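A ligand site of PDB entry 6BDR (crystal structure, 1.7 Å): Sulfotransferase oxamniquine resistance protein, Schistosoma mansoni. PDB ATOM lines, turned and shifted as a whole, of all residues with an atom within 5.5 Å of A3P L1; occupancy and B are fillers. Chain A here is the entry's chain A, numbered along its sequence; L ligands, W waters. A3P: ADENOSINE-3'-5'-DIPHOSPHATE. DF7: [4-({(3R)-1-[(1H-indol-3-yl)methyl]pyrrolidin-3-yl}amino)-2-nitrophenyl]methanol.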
ATOM      1  N   LEU A  17      28.833 -28.011 -37.651  1.00  0.00           N
ATOM      2  CA  LEU A  17      28.184 -29.306 -37.483  1.00  0.00           C
ATOM      3  C   LEU A  17      27.182 -29.283 -36.340  1.00  0.00           C
ATOM      4  O   LEU A  17      27.195 -28.374 -35.500  1.00  0.00           O
ATOM      5  CB  LEU A  17      29.245 -30.374 -37.245  1.00  0.00           C
ATOM      6  CG  LEU A  17      30.155 -30.608 -38.439  1.00  0.00           C
ATOM      7  CD1 LEU A  17      31.402 -31.330 -37.966  1.00  0.00           C
ATOM      8  CD2 LEU A  17      29.435 -31.395 -39.535  1.00  0.00           C
ATOM      9  N   PRO A  18      26.264 -30.228 -36.306  1.00  0.00           N
ATOM     10  CA  PRO A  18      25.349 -30.285 -35.154  1.00  0.00           C
ATOM     11  C   PRO A  18      26.120 -30.414 -33.854  1.00  0.00           C
ATOM     12  O   PRO A  18      27.211 -30.963 -33.805  1.00  0.00           O
ATOM     13  CB  PRO A  18      24.503 -31.535 -35.439  1.00  0.00           C
ATOM     14  CG  PRO A  18      25.158 -32.229 -36.543  1.00  0.00           C
ATOM     15  CD  PRO A  18      25.963 -31.266 -37.308  1.00  0.00           C
ATOM     16  N   ARG A  19      25.527 -29.843 -32.822  1.00  0.00           N
ATOM     17  CA  ARG A  19      26.053 -29.832 -31.444  1.00  0.00           C
ATOM     18  C   ARG A  19      27.227 -28.873 -31.292  1.00  0.00           C
ATOM     19  O   ARG A  19      28.071 -29.066 -30.407  1.00  0.00           O
ATOM     20  CB  ARG A  19      26.434 -31.233 -30.973  1.00  0.00           C
ATOM     21  CG  ARG A  19      25.356 -32.286 -31.184  1.00  0.00           C
ATOM     22  CD  ARG A  19      23.953 -31.875 -30.661  1.00  0.00           C
ATOM     23  NE  ARG A  19      23.915 -31.616 -29.219  1.00  0.00           N
ATOM     24  CZ  ARG A  19      22.892 -31.084 -28.561  1.00  0.00           C
ATOM     25  NH1 ARG A  19      21.814 -30.669 -29.201  1.00  0.00           N
ATOM     26  NH2 ARG A  19      22.964 -30.921 -27.246  1.00  0.00           N
ATOM     27  N   THR A  20      27.270 -27.833 -32.128  1.00  0.00           N
ATOM     28  CA  THR A  20      28.252 -26.760 -32.009  1.00  0.00           C
ATOM     29  C   THR A  20      27.609 -25.402 -31.752  1.00  0.00           C
ATOM     30  O   THR A  20      28.229 -24.363 -32.021  1.00  0.00           O
ATOM     31  CB  THR A  20      29.137 -26.670 -33.257  1.00  0.00           C
ATOM     32  OG1 THR A  20      28.365 -26.337 -34.414  1.00  0.00           O
ATOM     33  CG2 THR A  20      29.889 -27.952 -33.492  1.00  0.00           C
ATOM     34  N   GLY A  21      26.383 -25.376 -31.228  1.00  0.00           N
ATOM     35  CA  GLY A  21      25.694 -24.117 -31.013  1.00  0.00           C
ATOM     36  C   GLY A  21      24.820 -23.659 -32.154  1.00  0.00           C
ATOM     37  O   GLY A  21      24.508 -22.462 -32.227  1.00  0.00           O
ATOM     38  N   THR A  22      24.362 -24.586 -33.016  1.00  0.00           N
ATOM     39  CA  THR A  22      23.602 -24.199 -34.201  1.00  0.00           C
ATOM     40  C   THR A  22      22.218 -23.662 -33.842  1.00  0.00           C
ATOM     41  O   THR A  22      21.706 -22.759 -34.509  1.00  0.00           O
ATOM     42  CB  THR A  22      23.425 -25.369 -35.191  1.00  0.00           C
ATOM     43  OG1 THR A  22      22.661 -26.426 -34.598  1.00  0.00           O
ATOM     44  CG2 THR A  22      24.747 -25.927 -35.658  1.00  0.00           C
ATOM     45  N   LYS A  23      21.569 -24.219 -32.815  1.00  0.00           N
ATOM     46  CA  LYS A  23      20.225 -23.755 -32.498  1.00  0.00           C
ATOM     47  C   LYS A  23      20.266 -22.381 -31.869  1.00  0.00           C
ATOM     48  O   LYS A  23      19.420 -21.540 -32.136  1.00  0.00           O
ATOM     49  CB  LYS A  23      19.492 -24.733 -31.569  1.00  0.00           C
ATOM     50  CG  LYS A  23      18.023 -24.370 -31.261  1.00  0.00           C
ATOM     51  CD  LYS A  23      17.199 -24.208 -32.526  1.00  0.00           C
ATOM     52  CE  LYS A  23      15.694 -24.264 -32.269  1.00  0.00           C
ATOM     53  NZ  LYS A  23      15.116 -23.077 -31.603  1.00  0.00           N
ATOM     54  N   SER A  24      21.265 -22.130 -31.012  1.00  0.00           N
ATOM     55  CA  SER A  24      21.401 -20.801 -30.444  1.00  0.00           C
ATOM     56  C   SER A  24      21.695 -19.796 -31.554  1.00  0.00           C
ATOM     57  O   SER A  24      21.164 -18.683 -31.544  1.00  0.00           O
ATOM     58  CB  SER A  24      22.515 -20.767 -29.402  1.00  0.00           C
ATOM     59  OG  SER A  24      22.116 -21.488 -28.244  1.00  0.00           O
ATOM     60  N   HIS A  39      17.287 -25.005 -40.045  1.00  0.00           N
ATOM     61  CA  HIS A  39      17.871 -25.801 -38.962  1.00  0.00           C
ATOM     62  C   HIS A  39      17.181 -27.149 -39.026  1.00  0.00           C
ATOM     63  O   HIS A  39      16.077 -27.246 -39.555  1.00  0.00           O
ATOM     64  CB  HIS A  39      17.638 -25.141 -37.602  1.00  0.00           C
ATOM     65  CG  HIS A  39      18.403 -25.757 -36.477  1.00  0.00           C
ATOM     66  ND1 HIS A  39      17.909 -26.805 -35.735  1.00  0.00           N
ATOM     67  CD2 HIS A  39      19.602 -25.445 -35.943  1.00  0.00           C
ATOM     68  CE1 HIS A  39      18.783 -27.130 -34.805  1.00  0.00           C
ATOM     69  NE2 HIS A  39      19.829 -26.328 -34.908  1.00  0.00           N
ATOM     70  N   ASP A  93      23.059 -26.058 -39.417  1.00  0.00           N
ATOM     71  CA  ASP A  93      22.824 -27.436 -39.013  1.00  0.00           C
ATOM     72  C   ASP A  93      22.762 -28.392 -40.183  1.00  0.00           C
ATOM     73  O   ASP A  93      22.729 -27.971 -41.354  1.00  0.00           O
ATOM     74  CB  ASP A  93      21.494 -27.491 -38.244  1.00  0.00           C
ATOM     75  CG  ASP A  93      21.382 -28.665 -37.314  1.00  0.00           C
ATOM     76  OD1 ASP A  93      22.382 -29.412 -37.127  1.00  0.00           O
ATOM     77  OD2 ASP A  93      20.258 -28.827 -36.739  1.00  0.00           O
ATOM     78  N   ARG A 117      33.903 -26.247 -31.509  1.00  0.00           N
ATOM     79  CA  ARG A 117      34.106 -26.445 -30.086  1.00  0.00           C
ATOM     80  C   ARG A 117      35.087 -27.580 -29.871  1.00  0.00           C
ATOM     81  O   ARG A 117      35.496 -28.271 -30.812  1.00  0.00           O
ATOM     82  CB  ARG A 117      32.770 -26.739 -29.390  1.00  0.00           C
ATOM     83  CG  ARG A 117      32.277 -28.165 -29.646  1.00  0.00           C
ATOM     84  CD  ARG A 117      30.878 -28.408 -29.131  1.00  0.00           C
ATOM     85  NE  ARG A 117      30.792 -28.415 -27.671  1.00  0.00           N
ATOM     86  CZ  ARG A 117      29.708 -28.770 -26.994  1.00  0.00           C
ATOM     87  NH1 ARG A 117      28.616 -29.169 -27.643  1.00  0.00           N
ATOM     88  NH2 ARG A 117      29.722 -28.714 -25.666  1.00  0.00           N
ATOM     89  N   ASP A 121      33.998 -32.683 -26.213  1.00  0.00           N
ATOM     90  CA  ASP A 121      32.699 -32.163 -25.811  1.00  0.00           C
ATOM     91  C   ASP A 121      31.690 -32.360 -26.920  1.00  0.00           C
ATOM     92  O   ASP A 121      30.518 -32.675 -26.666  1.00  0.00           O
ATOM     93  CB  ASP A 121      32.748 -30.678 -25.455  1.00  0.00           C
ATOM     94  CG  ASP A 121      33.528 -30.367 -24.181  1.00  0.00           C
ATOM     95  OD1 ASP A 121      33.762 -31.267 -23.339  1.00  0.00           O
ATOM     96  OD2 ASP A 121      33.861 -29.167 -24.027  1.00  0.00           O
ATOM     97  N   SER A 125      28.269 -34.702 -26.709  1.00  0.00           N
ATOM     98  CA  SER A 125      26.958 -34.118 -26.974  1.00  0.00           C
ATOM     99  C   SER A 125      26.265 -34.861 -28.106  1.00  0.00           C
ATOM    100  O   SER A 125      25.063 -35.173 -28.043  1.00  0.00           O
ATOM    101  CB  SER A 125      27.152 -32.641 -27.336  1.00  0.00           C
ATOM    102  OG  SER A 125      25.937 -31.921 -27.464  1.00  0.00           O
ATOM    103  N   VAL A 129      22.501 -37.067 -28.064  1.00  0.00           N
ATOM    104  CA  VAL A 129      21.346 -36.457 -28.709  1.00  0.00           C
ATOM    105  C   VAL A 129      21.095 -36.991 -30.120  1.00  0.00           C
ATOM    106  O   VAL A 129      19.970 -37.394 -30.457  1.00  0.00           O
ATOM    107  CB  VAL A 129      21.521 -34.936 -28.757  1.00  0.00           C
ATOM    108  CG1 VAL A 129      20.372 -34.285 -29.532  1.00  0.00           C
ATOM    109  CG2 VAL A 129      21.612 -34.381 -27.347  1.00  0.00           C
ATOM    110  N   LEU A 205      31.872 -21.578 -29.085  1.00  0.00           N
ATOM    111  CA  LEU A 205      30.788 -21.463 -28.105  1.00  0.00           C
ATOM    112  C   LEU A 205      31.183 -20.474 -27.033  1.00  0.00           C
ATOM    113  O   LEU A 205      32.292 -20.540 -26.505  1.00  0.00           O
ATOM    114  CB  LEU A 205      30.487 -22.807 -27.444  1.00  0.00           C
ATOM    115  CG  LEU A 205      29.796 -23.872 -28.249  1.00  0.00           C
ATOM    116  CD1 LEU A 205      29.693 -25.130 -27.416  1.00  0.00           C
ATOM    117  CD2 LEU A 205      28.408 -23.363 -28.648  1.00  0.00           C
ATOM    118  N   GLY A 206      30.268 -19.565 -26.708  1.00  0.00           N
ATOM    119  CA  GLY A 206      30.517 -18.529 -25.734  1.00  0.00           C
ATOM    120  C   GLY A 206      30.912 -17.185 -26.327  1.00  0.00           C
ATOM    121  O   GLY A 206      31.009 -16.215 -25.575  1.00  0.00           O
ATOM    122  N   TYR A 226      22.614 -13.287 -25.642  1.00  0.00           N
ATOM    123  CA  TYR A 226      22.858 -14.223 -26.726  1.00  0.00           C
ATOM    124  C   TYR A 226      22.259 -15.572 -26.351  1.00  0.00           C
ATOM    125  O   TYR A 226      22.427 -16.016 -25.203  1.00  0.00           O
ATOM    126  CB  TYR A 226      24.354 -14.352 -27.016  1.00  0.00           C
ATOM    127  CG  TYR A 226      24.628 -15.208 -28.244  1.00  0.00           C
ATOM    128  CD1 TYR A 226      24.687 -14.649 -29.515  1.00  0.00           C
ATOM    129  CD2 TYR A 226      24.760 -16.571 -28.124  1.00  0.00           C
ATOM    130  CE1 TYR A 226      24.929 -15.451 -30.638  1.00  0.00           C
ATOM    131  CE2 TYR A 226      24.990 -17.368 -29.227  1.00  0.00           C
ATOM    132  CZ  TYR A 226      25.055 -16.804 -30.491  1.00  0.00           C
ATOM    133  OH  TYR A 226      25.281 -17.625 -31.576  1.00  0.00           O
ATOM    134  N   PRO A 227      21.546 -16.223 -27.241  1.00  0.00           N
ATOM    135  CA  PRO A 227      20.898 -17.459 -26.855  1.00  0.00           C
ATOM    136  C   PRO A 227      21.810 -18.571 -26.331  1.00  0.00           C
ATOM    137  O   PRO A 227      22.880 -18.671 -26.729  1.00  0.00           O
ATOM    138  CB  PRO A 227      20.175 -17.891 -28.114  1.00  0.00           C
ATOM    139  CG  PRO A 227      19.990 -16.662 -28.887  1.00  0.00           C
ATOM    140  CD  PRO A 227      21.153 -15.801 -28.581  1.00  0.00           C
ATOM    141  N   CAS A 228      21.261 -19.362 -25.436  1.00  0.00           N
ATOM    142  CA  CAS A 228      21.913 -20.502 -24.845  1.00  0.00           C
ATOM    143  CB  CAS A 228      22.558 -20.207 -23.482  1.00  0.00           C
ATOM    144  C   CAS A 228      20.853 -21.557 -24.715  1.00  0.00           C
ATOM    145  O   CAS A 228      20.154 -21.574 -23.758  1.00  0.00           O
ATOM    146  SG  CAS A 228      23.535 -21.579 -22.961  1.00  0.00           S
ATOM    147 AS   CAS A 228      22.223 -23.024 -21.653  1.00  0.00          AS
ATOM    148  CE1 CAS A 228      21.021 -24.359 -22.413  1.00  0.00           C
ATOM    149  CE2 CAS A 228      23.574 -24.259 -20.874  1.00  0.00           C
ATOM    150  N   VAL A 229      20.666 -22.372 -25.732  1.00  0.00           N
ATOM    151  CA  VAL A 229      19.649 -23.381 -25.736  1.00  0.00           C
ATOM    152  C   VAL A 229      20.140 -24.706 -26.318  1.00  0.00           C
ATOM    153  O   VAL A 229      21.182 -24.745 -26.860  1.00  0.00           O
ATOM    154  CB  VAL A 229      18.459 -22.955 -26.621  1.00  0.00           C
ATOM    155  CG1 VAL A 229      17.787 -21.728 -26.089  1.00  0.00           C
ATOM    156  CG2 VAL A 229      18.905 -22.702 -28.036  1.00  0.00           C
ATOM    157  N   ASN A 230      19.377 -25.766 -26.122  1.00  0.00           N
ATOM    158  CA  ASN A 230      19.662 -27.056 -26.763  1.00  0.00           C
ATOM    159  C   ASN A 230      20.845 -27.792 -26.133  1.00  0.00           C
ATOM    160  O   ASN A 230      21.541 -28.564 -26.824  1.00  0.00           O
ATOM    161  CB  ASN A 230      19.900 -26.859 -28.277  1.00  0.00           C
ATOM    162  CG  ASN A 230      19.546 -28.105 -29.079  1.00  0.00           C
ATOM    163  OD1 ASN A 230      18.930 -29.039 -28.581  1.00  0.00           O
ATOM    164  ND2 ASN A 230      19.957 -28.131 -30.336  1.00  0.00           N
ATOM    165  N   SER A 231      21.043 -27.663 -24.825  1.00  0.00           N
ATOM    166  CA  SER A 231      22.021 -28.495 -24.144  1.00  0.00           C
ATOM    167  C   SER A 231      21.557 -29.943 -24.168  1.00  0.00           C
ATOM    168  O   SER A 231      20.373 -30.218 -24.255  1.00  0.00           O
ATOM    169  CB  SER A 231      22.208 -28.060 -22.692  1.00  0.00           C
ATOM    170  OG  SER A 231      21.062 -28.352 -21.906  1.00  0.00           O
ATOM    171  N   HIS A 232      22.503 -30.878 -24.078  1.00  0.00           N
ATOM    172  CA  HIS A 232      22.055 -32.255 -24.088  1.00  0.00           C
ATOM    173  C   HIS A 232      21.203 -32.578 -22.863  1.00  0.00           C
ATOM    174  O   HIS A 232      20.293 -33.395 -22.942  1.00  0.00           O
ATOM    175  CB  HIS A 232      23.236 -33.220 -24.234  1.00  0.00           C
ATOM    176  CG  HIS A 232      24.157 -33.297 -23.056  1.00  0.00           C
ATOM    177  ND1 HIS A 232      23.855 -34.003 -21.913  1.00  0.00           N
ATOM    178  CD2 HIS A 232      25.401 -32.789 -22.878  1.00  0.00           C
ATOM    179  CE1 HIS A 232      24.864 -33.903 -21.056  1.00  0.00           C
ATOM    180  NE2 HIS A 232      25.810 -33.156 -21.613  1.00  0.00           N
ATOM    181  N   HIS A 233      21.464 -31.918 -21.736  1.00  0.00           N
ATOM    182  CA  HIS A 233      20.608 -32.112 -20.574  1.00  0.00           C
ATOM    183  C   HIS A 233      19.179 -31.711 -20.873  1.00  0.00           C
ATOM    184  O   HIS A 233      18.227 -32.385 -20.456  1.00  0.00           O
ATOM    185  CB  HIS A 233      21.140 -31.314 -19.379  1.00  0.00           C
ATOM    186  CG  HIS A 233      22.435 -31.817 -18.853  1.00  0.00           C
ATOM    187  ND1 HIS A 233      22.572 -33.065 -18.285  1.00  0.00           N
ATOM    188  CD2 HIS A 233      23.652 -31.231 -18.760  1.00  0.00           C
ATOM    189  CE1 HIS A 233      23.822 -33.234 -17.890  1.00  0.00           C
ATOM    190  NE2 HIS A 233      24.492 -32.142 -18.161  1.00  0.00           N
HETATM  191  P1  A3P L   1      25.999 -29.562 -24.829  1.00  0.00           P
HETATM  192  O1P A3P L   1      27.440 -29.988 -24.580  1.00  0.00           O
HETATM  193  O2P A3P L   1      25.109 -30.649 -25.394  1.00  0.00           O
HETATM  194  O3P A3P L   1      25.341 -28.898 -23.647  1.00  0.00           O
HETATM  195  P2  A3P L   1      23.335 -27.515 -31.352  1.00  0.00           P
HETATM  196  O4P A3P L   1      24.207 -27.293 -32.559  1.00  0.00           O
HETATM  197  O5P A3P L   1      22.278 -26.480 -31.120  1.00  0.00           O
HETATM  198  O6P A3P L   1      22.810 -28.940 -31.272  1.00  0.00           O
HETATM  199  O5' A3P L   1      24.393 -27.290 -30.144  1.00  0.00           O
HETATM  200  C5' A3P L   1      24.004 -27.478 -28.801  1.00  0.00           C
HETATM  201  C4' A3P L   1      25.256 -27.429 -27.919  1.00  0.00           C
HETATM  202  O4' A3P L   1      25.793 -26.094 -27.882  1.00  0.00           O
HETATM  203  C3' A3P L   1      24.952 -27.785 -26.481  1.00  0.00           C
HETATM  204  O3' A3P L   1      26.112 -28.396 -25.924  1.00  0.00           O
HETATM  205  C2' A3P L   1      24.747 -26.416 -25.854  1.00  0.00           C
HETATM  206  O2' A3P L   1      24.825 -26.470 -24.409  1.00  0.00           O
HETATM  207  C1' A3P L   1      25.852 -25.640 -26.512  1.00  0.00           C
HETATM  208  N9  A3P L   1      25.552 -24.186 -26.469  1.00  0.00           N
HETATM  209  C8  A3P L   1      24.537 -23.624 -27.152  1.00  0.00           C
HETATM  210  N7  A3P L   1      24.519 -22.280 -26.968  1.00  0.00           N
HETATM  211  C5  A3P L   1      25.531 -21.971 -26.115  1.00  0.00           C
HETATM  212  C6  A3P L   1      26.059 -20.752 -25.504  1.00  0.00           C
HETATM  213  N6  A3P L   1      25.464 -19.556 -25.735  1.00  0.00           N
HETATM  214  N1  A3P L   1      27.157 -20.871 -24.693  1.00  0.00           N
HETATM  215  C2  A3P L   1      27.725 -22.067 -24.469  1.00  0.00           C
HETATM  216  N3  A3P L   1      27.279 -23.226 -24.998  1.00  0.00           N
HETATM  217  C4  A3P L   1      26.209 -23.233 -25.823  1.00  0.00           C
HETATM  218  C1  DF7 L   2      18.889 -32.487 -34.040  1.00  0.00           C
HETATM  219  C2  DF7 L   2      19.823 -32.707 -35.021  1.00  0.00           C
HETATM  220  C3  DF7 L   2      19.954 -33.950 -35.627  1.00  0.00           C
HETATM  221  C4  DF7 L   2      19.111 -34.994 -35.236  1.00  0.00           C
HETATM  222  C5  DF7 L   2      18.185 -34.757 -34.229  1.00  0.00           C
HETATM  223  C6  DF7 L   2      18.065 -33.526 -33.638  1.00  0.00           C
HETATM  224  C21 DF7 L   2      20.029 -41.588 -35.658  1.00  0.00           C
HETATM  225  C14 DF7 L   2      16.926 -37.570 -32.483  1.00  0.00           C
HETATM  226  O9  DF7 L   2      20.030 -30.362 -34.856  1.00  0.00           O
HETATM  227  O10 DF7 L   2      20.622 -35.069 -37.482  1.00  0.00           O
HETATM  228  O11 DF7 L   2      21.984 -33.585 -36.743  1.00  0.00           O
HETATM  229  C19 DF7 L   2      19.995 -43.845 -36.609  1.00  0.00           C
HETATM  230  C20 DF7 L   2      20.385 -42.495 -36.665  1.00  0.00           C
HETATM  231  C16 DF7 L   2      19.270 -42.073 -34.604  1.00  0.00           C
HETATM  232  C17 DF7 L   2      18.380 -37.953 -34.309  1.00  0.00           C
HETATM  233  C18 DF7 L   2      19.231 -44.359 -35.562  1.00  0.00           C
HETATM  234  C15 DF7 L   2      16.895 -39.034 -32.824  1.00  0.00           C
HETATM  235  C12 DF7 L   2      18.861 -43.477 -34.557  1.00  0.00           C
HETATM  236  C10 DF7 L   2      18.009 -42.442 -32.647  1.00  0.00           C
HETATM  237  C7  DF7 L   2      20.678 -31.519 -35.383  1.00  0.00           C
HETATM  238  C8  DF7 L   2      18.865 -40.013 -33.030  1.00  0.00           C
HETATM  239  C9  DF7 L   2      18.697 -41.459 -33.373  1.00  0.00           C
HETATM  240  C13 DF7 L   2      17.216 -37.066 -33.873  1.00  0.00           C
HETATM  241  N11 DF7 L   2      18.091 -43.759 -33.380  1.00  0.00           N
HETATM  242  N12 DF7 L   2      17.315 -35.635 -33.735  1.00  0.00           N
HETATM  243  N16 DF7 L   2      17.908 -39.269 -33.829  1.00  0.00           N
HETATM  244  N8  DF7 L   2      20.897 -34.196 -36.641  1.00  0.00           N
HETATM  245  O   HOH W   1      28.854 -25.176 -23.484  1.00  0.00           O
HETATM  246  O   HOH W   2      26.835 -16.805 -25.152  1.00  0.00           O
HETATM  247  O   HOH W   3      29.189 -32.059 -24.190  1.00  0.00           O
HETATM  248  O   HOH W   4      20.768 -30.335 -32.253  1.00  0.00           O
HETATM  249  O   HOH W   5      28.187 -19.225 -22.873  1.00  0.00           O
HETATM  250  O   HOH W   6      22.503 -24.367 -29.579  1.00  0.00           O
HETATM  251  O   HOH W   7      25.188 -29.295 -21.128  1.00  0.00           O
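OG of Ser 125 lies within hydrogen-bond range of NE of Arg 19, at 2.7 Å. The side-chain hydroxyl (OG1) of Thr 20 sits at hydrogen-bond distance from the backbone carbonyl oxygen (O) of Leu 17, 2.6 Å away. The backbone carbonyl oxygen (O) of Asn 230 sits at hydrogen-bond distance from the guanidinium group (NH2) of Arg 19 (2.8 Å). OG of Ser 24 is in hydrogen-bond range of N of Val 229, at 3.0 Å. The side-chain hydroxyl (OG) of Ser 24 sits at hydrogen-bond distance from the backbone carbonyl oxygen (O) of Pro 227 (3.3 Å). The guanidinium group of Arg 117 lies within hydrogen-bond range of the backbone carbonyl oxygen of Arg 19 (2.8 Å). The side-chain hydroxyl of Thr 22 sits at hydrogen-bond distance from a ring nitrogen (NE2) of His 39, at 2.9 Å. A ring nitrogen (NE2) of His 39 lies within hydrogen-bond range of the backbone NH of Lys 23, 3.4 Å away.
OG of Ser 24 is in hydrogen-bond range of N7 of A3P L1 (2.8 Å). The side-chain hydroxyl (OG) of Ser 125 lies within hydrogen-bond range of an oxygen (O2P) of A3P L1, 2.6 Å away. The side-chain amide nitrogen (ND2) of Asn 230 lies within hydrogen-bond range of an oxygen (O5P) of A3P L1, at 3.0 Å. A nitrogen (N6) of A3P L1 is in hydrogen-bond range of the backbone carbonyl oxygen (O) of Pro 227. The backbone NH of Arg 19 is in hydrogen-bond range of an oxygen (O4P) of A3P L1. O2P of A3P L1 lies within hydrogen-bond range of N of His 232 (2.9 Å). The guanidinium group of Arg 19 lies within salt-bridge range of an oxygen (O2P) of A3P L1 (2.8 Å). OG1 of Thr 22 is in hydrogen-bond range of O4P of A3P L1, at 2.7 Å. The side-chain carboxylate of Asp 93 lies within hydrogen-bond range of an oxygen (O9) of DF7 L2 (2.4 Å). O4P of A3P L1 lies within hydrogen-bond range of N of Thr 22, 2.7 Å away. An oxygen (O5P) of A3P L1 is in hydrogen-bond range of the backbone NH (N) of Lys 23 (2.9 Å). An oxygen (O4P) of A3P L1 sits at hydrogen-bond distance from the backbone NH (N) of Thr 20, 3.1 Å away. The guanidinium group (NH2) of Arg 117 is in salt-bridge range of an oxygen (O1P) of A3P L1. The backbone NH (N) of Gly 21 is in hydrogen-bond range of an oxygen (O5') of A3P L1 (3.0 Å).
Residues that only touch A3P L1: Pro 18, Leu 205, Gly 206, Tyr 226, CAS 228, Val 229 and Ser 231. Within 4 Å of A3P L1: Pro 18, Arg 19, Thr 20, Gly 21, Thr 22, Lys 23, Ser 24, Arg 117, Ser 125, Leu 205, Gly 206, Tyr 226, Pro 227, CAS 228, Val 229, Asn 230, Ser 231 and His 232.
Water W6 lies within hydrogen-bond range of O5P of A3P L1, N of Ser 24, O of Val 229 and N of Lys 23. Water W4 lies within hydrogen-bond range of an oxygen (O6P) of A3P L1 (2.7 Å), an oxygen (O9) of DF7 L2 (2.7 Å), the side-chain amide nitrogen of Asn 230 (3.0 Å) and the guanidinium group of Arg 19 (3.2 Å). Water W3 lies within hydrogen-bond range of an oxygen (O1P) of A3P L1 (2.7 Å) and the backbone carbonyl oxygen (O) of Asp 121 (2.9 Å).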
